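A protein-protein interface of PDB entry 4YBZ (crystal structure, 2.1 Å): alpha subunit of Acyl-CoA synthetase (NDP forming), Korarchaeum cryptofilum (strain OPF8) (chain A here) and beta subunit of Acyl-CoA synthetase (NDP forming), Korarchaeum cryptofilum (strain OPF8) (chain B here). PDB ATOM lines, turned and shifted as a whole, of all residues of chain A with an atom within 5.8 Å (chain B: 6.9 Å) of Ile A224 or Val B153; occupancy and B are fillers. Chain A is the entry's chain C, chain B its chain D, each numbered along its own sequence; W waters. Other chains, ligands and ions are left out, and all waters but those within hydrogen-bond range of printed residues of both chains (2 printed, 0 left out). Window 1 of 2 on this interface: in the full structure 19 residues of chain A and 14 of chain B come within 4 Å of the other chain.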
ATOM      1  N   ARG A 219      14.128 -11.789  29.050  1.00  0.00           N
ATOM      2  CA  ARG A 219      14.149 -13.249  28.977  1.00  0.00           C
ATOM      3  C   ARG A 219      13.019 -13.800  28.108  1.00  0.00           C
ATOM      4  O   ARG A 219      13.040 -14.965  27.700  1.00  0.00           O
ATOM      5  CB  ARG A 219      14.042 -13.835  30.385  1.00  0.00           C
ATOM      6  CG  ARG A 219      14.535 -15.260  30.513  1.00  0.00           C
ATOM      7  CD  ARG A 219      16.044 -15.316  30.428  1.00  0.00           C
ATOM      8  NE  ARG A 219      16.546 -16.682  30.550  1.00  0.00           N
ATOM      9  CZ  ARG A 219      17.551 -17.187  29.843  1.00  0.00           C
ATOM     10  NH1 ARG A 219      18.184 -16.453  28.936  1.00  0.00           N
ATOM     11  NH2 ARG A 219      17.926 -18.444  30.041  1.00  0.00           N
ATOM     12  N   GLY A 220      12.042 -12.950  27.820  1.00  0.00           N
ATOM     13  CA  GLY A 220      10.814 -13.369  27.176  1.00  0.00           C
ATOM     14  C   GLY A 220      10.923 -13.961  25.787  1.00  0.00           C
ATOM     15  O   GLY A 220      10.279 -14.967  25.491  1.00  0.00           O
ATOM     16  N   ARG A 221      11.716 -13.343  24.920  1.00  0.00           N
ATOM     17  CA  ARG A 221      11.800 -13.815  23.546  1.00  0.00           C
ATOM     18  C   ARG A 221      12.428 -15.204  23.484  1.00  0.00           C
ATOM     19  O   ARG A 221      11.952 -16.076  22.753  1.00  0.00           O
ATOM     20  CB  ARG A 221      12.594 -12.833  22.677  1.00  0.00           C
ATOM     21  CG  ARG A 221      12.605 -13.186  21.191  1.00  0.00           C
ATOM     22  CD  ARG A 221      11.203 -13.150  20.583  1.00  0.00           C
ATOM     23  NE  ARG A 221      10.917 -14.338  19.782  1.00  0.00           N
ATOM     24  CZ  ARG A 221       9.759 -14.566  19.170  1.00  0.00           C
ATOM     25  NH1 ARG A 221       8.765 -13.692  19.264  1.00  0.00           N
ATOM     26  NH2 ARG A 221       9.591 -15.674  18.462  1.00  0.00           N
ATOM     27  N   MET A 222      13.491 -15.412  24.252  1.00  0.00           N
ATOM     28  CA  MET A 222      14.128 -16.720  24.305  1.00  0.00           C
ATOM     29  C   MET A 222      13.157 -17.735  24.909  1.00  0.00           C
ATOM     30  O   MET A 222      13.138 -18.895  24.501  1.00  0.00           O
ATOM     31  CB  MET A 222      15.435 -16.670  25.095  1.00  0.00           C
ATOM     32  CG  MET A 222      16.404 -17.776  24.696  1.00  0.00           C
ATOM     33  SD  MET A 222      18.083 -17.512  25.298  1.00  0.00           S
ATOM     34  CE  MET A 222      18.071 -18.549  26.752  1.00  0.00           C
ATOM     35  N   PHE A 223      12.373 -17.301  25.895  1.00  0.00           N
ATOM     36  CA  PHE A 223      11.341 -18.157  26.487  1.00  0.00           C
ATOM     37  C   PHE A 223      10.363 -18.635  25.418  1.00  0.00           C
ATOM     38  O   PHE A 223      10.001 -19.810  25.378  1.00  0.00           O
ATOM     39  CB  PHE A 223      10.592 -17.417  27.602  1.00  0.00           C
ATOM     40  CG  PHE A 223       9.467 -18.209  28.214  1.00  0.00           C
ATOM     41  CD1 PHE A 223       8.204 -18.194  27.637  1.00  0.00           C
ATOM     42  CD2 PHE A 223       9.661 -18.961  29.359  1.00  0.00           C
ATOM     43  CE1 PHE A 223       7.162 -18.912  28.187  1.00  0.00           C
ATOM     44  CE2 PHE A 223       8.617 -19.682  29.914  1.00  0.00           C
ATOM     45  CZ  PHE A 223       7.367 -19.657  29.323  1.00  0.00           C
ATOM     46  N   ILE A 224       9.943 -17.721  24.553  1.00  0.00           N
ATOM     47  CA  ILE A 224       9.038 -18.062  23.465  1.00  0.00           C
ATOM     48  C   ILE A 224       9.708 -19.006  22.472  1.00  0.00           C
ATOM     49  O   ILE A 224       9.094 -19.954  21.996  1.00  0.00           O
ATOM     50  CB  ILE A 224       8.549 -16.795  22.728  1.00  0.00           C
ATOM     51  CG1 ILE A 224       7.646 -15.975  23.655  1.00  0.00           C
ATOM     52  CG2 ILE A 224       7.792 -17.163  21.444  1.00  0.00           C
ATOM     53  CD1 ILE A 224       7.250 -14.622  23.111  1.00  0.00           C
ATOM     54  N   ASP A 225      10.967 -18.746  22.145  1.00  0.00           N
ATOM     55  CA  ASP A 225      11.662 -19.568  21.159  1.00  0.00           C
ATOM     56  C   ASP A 225      11.817 -21.002  21.655  1.00  0.00           C
ATOM     57  O   ASP A 225      11.506 -21.959  20.940  1.00  0.00           O
ATOM     58  CB  ASP A 225      13.035 -18.972  20.837  1.00  0.00           C
ATOM     59  CG  ASP A 225      12.939 -17.605  20.184  1.00  0.00           C
ATOM     60  OD1 ASP A 225      11.894 -17.308  19.569  1.00  0.00           O
ATOM     61  OD2 ASP A 225      13.912 -16.829  20.286  1.00  0.00           O
ATOM     62  N   VAL A 226      12.229 -21.152  22.908  1.00  0.00           N
ATOM     63  CA  VAL A 226      12.468 -22.477  23.471  1.00  0.00           C
ATOM     64  C   VAL A 226      11.154 -23.189  23.772  1.00  0.00           C
ATOM     65  O   VAL A 226      11.002 -24.371  23.478  1.00  0.00           O
ATOM     66  CB  VAL A 226      13.317 -22.402  24.752  1.00  0.00           C
ATOM     67  CG1 VAL A 226      13.489 -23.791  25.367  1.00  0.00           C
ATOM     68  CG2 VAL A 226      14.678 -21.796  24.441  1.00  0.00           C
ATOM     69  N   ALA A 227      10.206 -22.476  24.368  1.00  0.00           N
ATOM     70  CA  ALA A 227       8.930 -23.078  24.726  1.00  0.00           C
ATOM     71  C   ALA A 227       8.191 -23.548  23.477  1.00  0.00           C
ATOM     72  O   ALA A 227       7.505 -24.567  23.503  1.00  0.00           O
ATOM     73  CB  ALA A 227       8.077 -22.101  25.509  1.00  0.00           C
ATOM     74  N   SER A 228       8.280 -22.770  22.403  1.00  0.00           N
ATOM     75  CA  SER A 228       7.614 -23.142  21.158  1.00  0.00           C
ATOM     76  C   SER A 228       8.225 -24.413  20.573  1.00  0.00           C
ATOM     77  O   SER A 228       7.497 -25.331  20.197  1.00  0.00           O
ATOM     78  CB  SER A 228       7.686 -22.007  20.138  1.00  0.00           C
ATOM     79  OG  SER A 228       9.024 -21.709  19.796  1.00  0.00           O
ATOM     80  N   ARG A 229       9.556 -24.493  20.552  1.00  0.00           N
ATOM     81  CA  ARG A 229      10.223 -25.680  20.021  1.00  0.00           C
ATOM     82  C   ARG A 229       9.837 -26.902  20.854  1.00  0.00           C
ATOM     83  O   ARG A 229       9.526 -27.962  20.304  1.00  0.00           O
ATOM     84  CB  ARG A 229      11.752 -25.492  19.987  1.00  0.00           C
ATOM     85  CG  ARG A 229      12.525 -26.063  21.185  1.00  0.00           C
ATOM     86  CD  ARG A 229      14.032 -25.837  21.092  1.00  0.00           C
ATOM     87  NE  ARG A 229      14.390 -24.467  20.714  1.00  0.00           N
ATOM     88  CZ  ARG A 229      15.466 -23.814  21.143  1.00  0.00           C
ATOM     89  NH1 ARG A 229      16.317 -24.379  21.993  1.00  0.00           N
ATOM     90  NH2 ARG A 229      15.692 -22.574  20.728  1.00  0.00           N
ATOM     91  N   ILE A 264       0.443  -9.505  27.665  1.00  0.00           N
ATOM     92  CA  ILE A 264       1.569  -9.920  26.838  1.00  0.00           C
ATOM     93  C   ILE A 264       1.967 -11.339  27.214  1.00  0.00           C
ATOM     94  O   ILE A 264       2.352 -12.127  26.351  1.00  0.00           O
ATOM     95  CB  ILE A 264       2.799  -8.995  26.993  1.00  0.00           C
ATOM     96  CG1 ILE A 264       2.446  -7.524  26.733  1.00  0.00           C
ATOM     97  CG2 ILE A 264       3.932  -9.452  26.069  1.00  0.00           C
ATOM     98  CD1 ILE A 264       1.420  -7.275  25.650  1.00  0.00           C
ATOM     99  N   SER A 267      -0.335 -13.728  25.459  1.00  0.00           N
ATOM    100  CA  SER A 267      -0.024 -13.772  24.041  1.00  0.00           C
ATOM    101  C   SER A 267       1.232 -14.600  23.804  1.00  0.00           C
ATOM    102  O   SER A 267       1.300 -15.394  22.865  1.00  0.00           O
ATOM    103  CB  SER A 267       0.154 -12.356  23.505  1.00  0.00           C
ATOM    104  OG  SER A 267      -1.059 -11.635  23.627  1.00  0.00           O
ATOM    105  N   ALA A 268       2.223 -14.409  24.668  1.00  0.00           N
ATOM    106  CA  ALA A 268       3.457 -15.178  24.607  1.00  0.00           C
ATOM    107  C   ALA A 268       3.172 -16.660  24.817  1.00  0.00           C
ATOM    108  O   ALA A 268       3.803 -17.509  24.195  1.00  0.00           O
ATOM    109  CB  ALA A 268       4.452 -14.672  25.643  1.00  0.00           C
ATOM    110  N   GLN A 271       1.775 -17.994  21.531  1.00  0.00           N
ATOM    111  CA  GLN A 271       2.829 -18.157  20.531  1.00  0.00           C
ATOM    112  C   GLN A 271       3.761 -19.325  20.845  1.00  0.00           C
ATOM    113  O   GLN A 271       4.412 -19.857  19.947  1.00  0.00           O
ATOM    114  CB  GLN A 271       3.648 -16.876  20.399  1.00  0.00           C
ATOM    115  CG  GLN A 271       2.861 -15.701  19.859  1.00  0.00           C
ATOM    116  CD  GLN A 271       3.650 -14.415  19.898  1.00  0.00           C
ATOM    117  OE1 GLN A 271       3.386 -13.541  20.724  1.00  0.00           O
ATOM    118  NE2 GLN A 271       4.624 -14.289  19.003  1.00  0.00           N
ATOM    119  N   SER A 272       3.864 -19.672  22.126  1.00  0.00           N
ATOM    120  CA  SER A 272       4.708 -20.777  22.576  1.00  0.00           C
ATOM    121  C   SER A 272       4.007 -22.130  22.520  1.00  0.00           C
ATOM    122  O   SER A 272       4.638 -23.167  22.724  1.00  0.00           O
ATOM    123  CB  SER A 272       5.186 -20.523  24.002  1.00  0.00           C
ATOM    124  OG  SER A 272       5.941 -19.329  24.076  1.00  0.00           O
ATOM    125  N   ASP B 127       7.940  -4.289  25.796  1.00  0.00           N
ATOM    126  CA  ASP B 127       7.626  -4.864  27.090  1.00  0.00           C
ATOM    127  C   ASP B 127       8.934  -5.297  27.751  1.00  0.00           C
ATOM    128  O   ASP B 127       9.780  -5.876  27.078  1.00  0.00           O
ATOM    129  CB  ASP B 127       6.681  -6.053  26.930  1.00  0.00           C
ATOM    130  CG  ASP B 127       6.483  -6.819  28.218  1.00  0.00           C
ATOM    131  OD1 ASP B 127       5.604  -6.431  29.017  1.00  0.00           O
ATOM    132  OD2 ASP B 127       7.206  -7.814  28.425  1.00  0.00           O
ATOM    133  N   PHE B 130       9.406  -9.121  27.119  1.00  0.00           N
ATOM    134  CA  PHE B 130       9.330  -9.716  25.785  1.00  0.00           C
ATOM    135  C   PHE B 130       9.854  -8.855  24.634  1.00  0.00           C
ATOM    136  O   PHE B 130       9.849  -9.294  23.486  1.00  0.00           O
ATOM    137  CB  PHE B 130       7.878 -10.119  25.527  1.00  0.00           C
ATOM    138  CG  PHE B 130       7.417 -11.253  26.397  1.00  0.00           C
ATOM    139  CD1 PHE B 130       7.814 -12.551  26.125  1.00  0.00           C
ATOM    140  CD2 PHE B 130       6.629 -11.019  27.511  1.00  0.00           C
ATOM    141  CE1 PHE B 130       7.415 -13.599  26.930  1.00  0.00           C
ATOM    142  CE2 PHE B 130       6.224 -12.063  28.320  1.00  0.00           C
ATOM    143  CZ  PHE B 130       6.619 -13.356  28.030  1.00  0.00           C
ATOM    144  N   GLY B 131      10.311  -7.642  24.926  1.00  0.00           N
ATOM    145  CA  GLY B 131      10.870  -6.789  23.891  1.00  0.00           C
ATOM    146  C   GLY B 131       9.793  -6.279  22.950  1.00  0.00           C
ATOM    147  O   GLY B 131       8.631  -6.187  23.342  1.00  0.00           O
ATOM    148  N   PRO B 132      10.156  -5.980  21.689  1.00  0.00           N
ATOM    149  CA  PRO B 132       9.179  -5.348  20.791  1.00  0.00           C
ATOM    150  C   PRO B 132       7.913  -6.183  20.609  1.00  0.00           C
ATOM    151  O   PRO B 132       7.978  -7.356  20.244  1.00  0.00           O
ATOM    152  CB  PRO B 132       9.950  -5.214  19.474  1.00  0.00           C
ATOM    153  CG  PRO B 132      10.990  -6.274  19.538  1.00  0.00           C
ATOM    154  CD  PRO B 132      11.403  -6.317  20.980  1.00  0.00           C
ATOM    155  N   THR B 133       6.770  -5.555  20.868  1.00  0.00           N
ATOM    156  CA  THR B 133       5.476  -6.222  20.864  1.00  0.00           C
ATOM    157  C   THR B 133       4.490  -5.450  19.991  1.00  0.00           C
ATOM    158  O   THR B 133       4.306  -4.248  20.170  1.00  0.00           O
ATOM    159  CB  THR B 133       4.910  -6.337  22.293  1.00  0.00           C
ATOM    160  OG1 THR B 133       5.820  -7.080  23.116  1.00  0.00           O
ATOM    161  CG2 THR B 133       3.544  -7.013  22.290  1.00  0.00           C
ATOM    162  N   VAL B 134       3.851  -6.145  19.057  1.00  0.00           N
ATOM    163  CA  VAL B 134       2.891  -5.505  18.166  1.00  0.00           C
ATOM    164  C   VAL B 134       1.497  -5.552  18.780  1.00  0.00           C
ATOM    165  O   VAL B 134       1.077  -6.586  19.294  1.00  0.00           O
ATOM    166  CB  VAL B 134       2.866  -6.177  16.778  1.00  0.00           C
ATOM    167  CG1 VAL B 134       1.780  -5.563  15.896  1.00  0.00           C
ATOM    168  CG2 VAL B 134       4.227  -6.057  16.107  1.00  0.00           C
ATOM    169  N   PHE B 151      -2.201  -8.681  21.213  1.00  0.00           N
ATOM    170  CA  PHE B 151      -0.754  -8.492  21.192  1.00  0.00           C
ATOM    171  C   PHE B 151      -0.030  -9.706  20.636  1.00  0.00           C
ATOM    172  O   PHE B 151      -0.478 -10.833  20.816  1.00  0.00           O
ATOM    173  CB  PHE B 151      -0.224  -8.204  22.595  1.00  0.00           C
ATOM    174  CG  PHE B 151      -0.751  -6.942  23.204  1.00  0.00           C
ATOM    175  CD1 PHE B 151      -0.170  -5.722  22.912  1.00  0.00           C
ATOM    176  CD2 PHE B 151      -1.809  -6.979  24.096  1.00  0.00           C
ATOM    177  CE1 PHE B 151      -0.646  -4.561  23.484  1.00  0.00           C
ATOM    178  CE2 PHE B 151      -2.287  -5.820  24.671  1.00  0.00           C
ATOM    179  CZ  PHE B 151      -1.703  -4.610  24.364  1.00  0.00           C
ATOM    180  N   ARG B 152       1.074  -9.468  19.937  1.00  0.00           N
ATOM    181  CA  ARG B 152       2.008 -10.534  19.591  1.00  0.00           C
ATOM    182  C   ARG B 152       3.438 -10.027  19.729  1.00  0.00           C
ATOM    183  O   ARG B 152       3.745  -8.899  19.347  1.00  0.00           O
ATOM    184  CB  ARG B 152       1.767 -11.047  18.170  1.00  0.00           C
ATOM    185  CG  ARG B 152       0.427 -11.743  17.957  1.00  0.00           C
ATOM    186  CD  ARG B 152       0.388 -13.140  18.574  1.00  0.00           C
ATOM    187  NE  ARG B 152      -0.856 -13.823  18.230  1.00  0.00           N
ATOM    188  CZ  ARG B 152      -2.002 -13.699  18.890  1.00  0.00           C
ATOM    189  NH1 ARG B 152      -2.083 -12.935  19.970  1.00  0.00           N
ATOM    190  NH2 ARG B 152      -3.076 -14.355  18.480  1.00  0.00           N
ATOM    191  N   VAL B 153       4.306 -10.865  20.284  1.00  0.00           N
ATOM    192  CA  VAL B 153       5.710 -10.519  20.437  1.00  0.00           C
ATOM    193  C   VAL B 153       6.403 -10.691  19.094  1.00  0.00           C
ATOM    194  O   VAL B 153       6.241 -11.714  18.431  1.00  0.00           O
ATOM    195  CB  VAL B 153       6.405 -11.389  21.510  1.00  0.00           C
ATOM    196  CG1 VAL B 153       7.865 -10.974  21.682  1.00  0.00           C
ATOM    197  CG2 VAL B 153       5.658 -11.298  22.833  1.00  0.00           C
ATOM    198  N   ALA B 154       7.165  -9.678  18.695  1.00  0.00           N
ATOM    199  CA  ALA B 154       7.827  -9.678  17.398  1.00  0.00           C
ATOM    200  C   ALA B 154       9.108 -10.513  17.433  1.00  0.00           C
ATOM    201  O   ALA B 154       9.701 -10.685  18.498  1.00  0.00           O
ATOM    202  CB  ALA B 154       8.137  -8.250  16.971  1.00  0.00           C
ATOM    203  N   PRO B 155       9.550 -11.021  16.268  1.00  0.00           N
ATOM    204  CA  PRO B 155       8.913 -10.859  14.953  1.00  0.00           C
ATOM    205  C   PRO B 155       7.640 -11.686  14.808  1.00  0.00           C
ATOM    206  O   PRO B 155       7.527 -12.757  15.404  1.00  0.00           O
ATOM    207  CB  PRO B 155       9.993 -11.346  13.984  1.00  0.00           C
ATOM    208  CG  PRO B 155      10.778 -12.325  14.777  1.00  0.00           C
ATOM    209  CD  PRO B 155      10.834 -11.735  16.158  1.00  0.00           C
ATOM    210  N   LEU B 156       6.696 -11.184  14.018  1.00  0.00           N
ATOM    211  CA  LEU B 156       5.432 -11.872  13.792  1.00  0.00           C
ATOM    212  C   LEU B 156       5.505 -12.816  12.606  1.00  0.00           C
ATOM    213  O   LEU B 156       5.963 -12.442  11.527  1.00  0.00           O
ATOM    214  CB  LEU B 156       4.295 -10.876  13.555  1.00  0.00           C
ATOM    215  CG  LEU B 156       3.549 -10.350  14.781  1.00  0.00           C
ATOM    216  CD1 LEU B 156       4.484  -9.611  15.720  1.00  0.00           C
ATOM    217  CD2 LEU B 156       2.389  -9.472  14.351  1.00  0.00           C
ATOM    218  N   SER B 157       5.054 -14.045  12.819  1.00  0.00           N
ATOM    219  CA  SER B 157       4.805 -14.951  11.713  1.00  0.00           C
ATOM    220  C   SER B 157       3.471 -14.554  11.101  1.00  0.00           C
ATOM    221  O   SER B 157       2.711 -13.780  11.692  1.00  0.00           O
ATOM    222  CB  SER B 157       4.751 -16.402  12.183  1.00  0.00           C
ATOM    223  OG  SER B 157       3.539 -16.621  12.878  1.00  0.00           O
ATOM    224  N   ASP B 160       0.829 -15.523  13.493  1.00  0.00           N
ATOM    225  CA  ASP B 160       0.615 -14.543  14.556  1.00  0.00           C
ATOM    226  C   ASP B 160      -0.267 -13.395  14.082  1.00  0.00           C
ATOM    227  O   ASP B 160      -1.219 -13.013  14.762  1.00  0.00           O
ATOM    228  CB  ASP B 160       1.945 -13.988  15.064  1.00  0.00           C
ATOM    229  CG  ASP B 160       2.836 -15.055  15.640  1.00  0.00           C
ATOM    230  OD1 ASP B 160       2.325 -15.914  16.387  1.00  0.00           O
ATOM    231  OD2 ASP B 160       4.048 -15.040  15.344  1.00  0.00           O
ATOM    232  N   MET B 164      -4.098 -12.908  15.618  1.00  0.00           N
ATOM    233  CA  MET B 164      -4.283 -11.762  16.503  1.00  0.00           C
ATOM    234  C   MET B 164      -5.362 -10.834  15.943  1.00  0.00           C
ATOM    235  O   MET B 164      -6.048 -10.149  16.702  1.00  0.00           O
ATOM    236  CB  MET B 164      -2.967 -11.008  16.719  1.00  0.00           C
ATOM    237  CG  MET B 164      -2.628  -9.960  15.675  1.00  0.00           C
ATOM    238  SD  MET B 164      -0.960  -9.310  15.904  1.00  0.00           S
ATOM    239  CE  MET B 164      -1.185  -8.298  17.370  1.00  0.00           C
ATOM    240  N   GLY B 196       6.280  -5.152  13.281  1.00  0.00           N
ATOM    241  CA  GLY B 196       7.112  -5.977  14.137  1.00  0.00           C
ATOM    242  C   GLY B 196       8.574  -5.908  13.737  1.00  0.00           C
ATOM    243  O   GLY B 196       9.465  -5.843  14.588  1.00  0.00           O
ATOM    244  N   VAL B 200      11.864  -4.704  15.908  1.00  0.00           N
ATOM    245  CA  VAL B 200      12.984  -5.619  16.105  1.00  0.00           C
ATOM    246  C   VAL B 200      14.293  -5.019  15.613  1.00  0.00           C
ATOM    247  O   VAL B 200      15.304  -5.070  16.310  1.00  0.00           O
ATOM    248  CB  VAL B 200      12.728  -6.964  15.387  1.00  0.00           C
ATOM    249  CG1 VAL B 200      14.029  -7.755  15.187  1.00  0.00           C
ATOM    250  CG2 VAL B 200      11.718  -7.789  16.172  1.00  0.00           C
HETATM  251  O   HOH W   1      -3.652 -10.662  22.724  1.00  0.00           O
HETATM  252  O   HOH W   2       5.748 -16.329  16.923  1.00  0.00           O
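NH1 of Arg A221 lies within hydrogen-bond range of O of Val B153, at 3.3 Å.
The guanidinium group of Arg A221 lies within hydrogen-bond range of the backbone carbonyl oxygen of Ala B154, 3.2 Å away.
O of Phe B151 is in hydrogen-bond range of OG of Ser A267, 3.0 Å away.
OE1 of Gln A271 lies within hydrogen-bond range of N of Val B153, at 2.9 Å.
The guanidinium group (NH2) of Arg A221 lies within salt-bridge range of the side-chain carboxylate (OD1) of Asp A225 (3.0 Å).
The backbone carbonyl oxygen (O) of Ala A268 lies within hydrogen-bond range of the side-chain hydroxyl (OG) of Ser A272.
The backbone carbonyl oxygen (O) of Gly B131 lies within hydrogen-bond range of the side-chain hydroxyl (OG1) of Thr B133 (3.0 Å).
O of Pro B132 sits at hydrogen-bond distance from N of Ala B154 (2.9 Å).
The backbone NH (N) of Val B134 sits at hydrogen-bond distance from the backbone carbonyl oxygen (O) of Arg B152 (2.8 Å).
OD2 of Asp B160 sits at hydrogen-bond distance from N of Ser B157, 2.9 Å away.
Gly A220 touches Phe B130 (CA to CD1, 3.3 Å).
CD1 of Phe B130 touches CD1 of Ile A224, 3.7 Å away.
CD1 of Ile A224 touches CG2 of Val B153, 3.7 Å away.
CG2 of Ile A264 touches CD2 of Phe B130 (3.4 Å).
Ile A264 touches Thr B133.
Ile A264 touches Phe B151.
Phe B130 touches Ala A268 (CE1 to CB, 3.4 Å).
Gln A271 touches Arg B152.
CG of Gln A271 touches OD1 of Asp B160, 3.5 Å away.
Of the printed residues of chain B, Gly A220 touches Phe B130 (3.3 Å).
Of the printed residues of chain B, Arg A221 touches Val B153 and Ala B154.
Ser A272 touches none of the printed residues of chain B.
Printed residues of chain A within 4 Å of Arg B152: Gln A271 (3.5 Å).
Val B153 touches just these residues of chain A: Arg A221 (3.3 Å), Ile A224 (3.7 Å) and Gln A271 (2.9 Å).
Ser B157 touches none of the printed residues of chain A.
The nearest residue of chain A that does not touch Val B153 is Ile A264 (4.1 Å).
The nearest printed residue of chain A that does not touch Asp B160 is Arg A221 (6.3 Å).
Of the 17 printed residues of chain B, 7 touch a printed residue of chain A.
Printed residues of chain B that touch a printed residue of chain A: Phe B130, Thr B133, Phe B151, Arg B152, Val B153, Ala B154 and Asp B160.
Hydrophobic or aromatic side chains of chain A that line the printed part of chain B: Ile A224, Ile A264 and Ala A268.
Among the printed residues, 13 pairs touch across the chains.
Water W2 bridges the side-chain carboxylate of Asp B160 (2.7 Å) and the side-chain amide nitrogen of Gln A271 (3.1 Å).
Water W1 lies within hydrogen-bond range of N of Phe B151 and OG of Ser A267.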
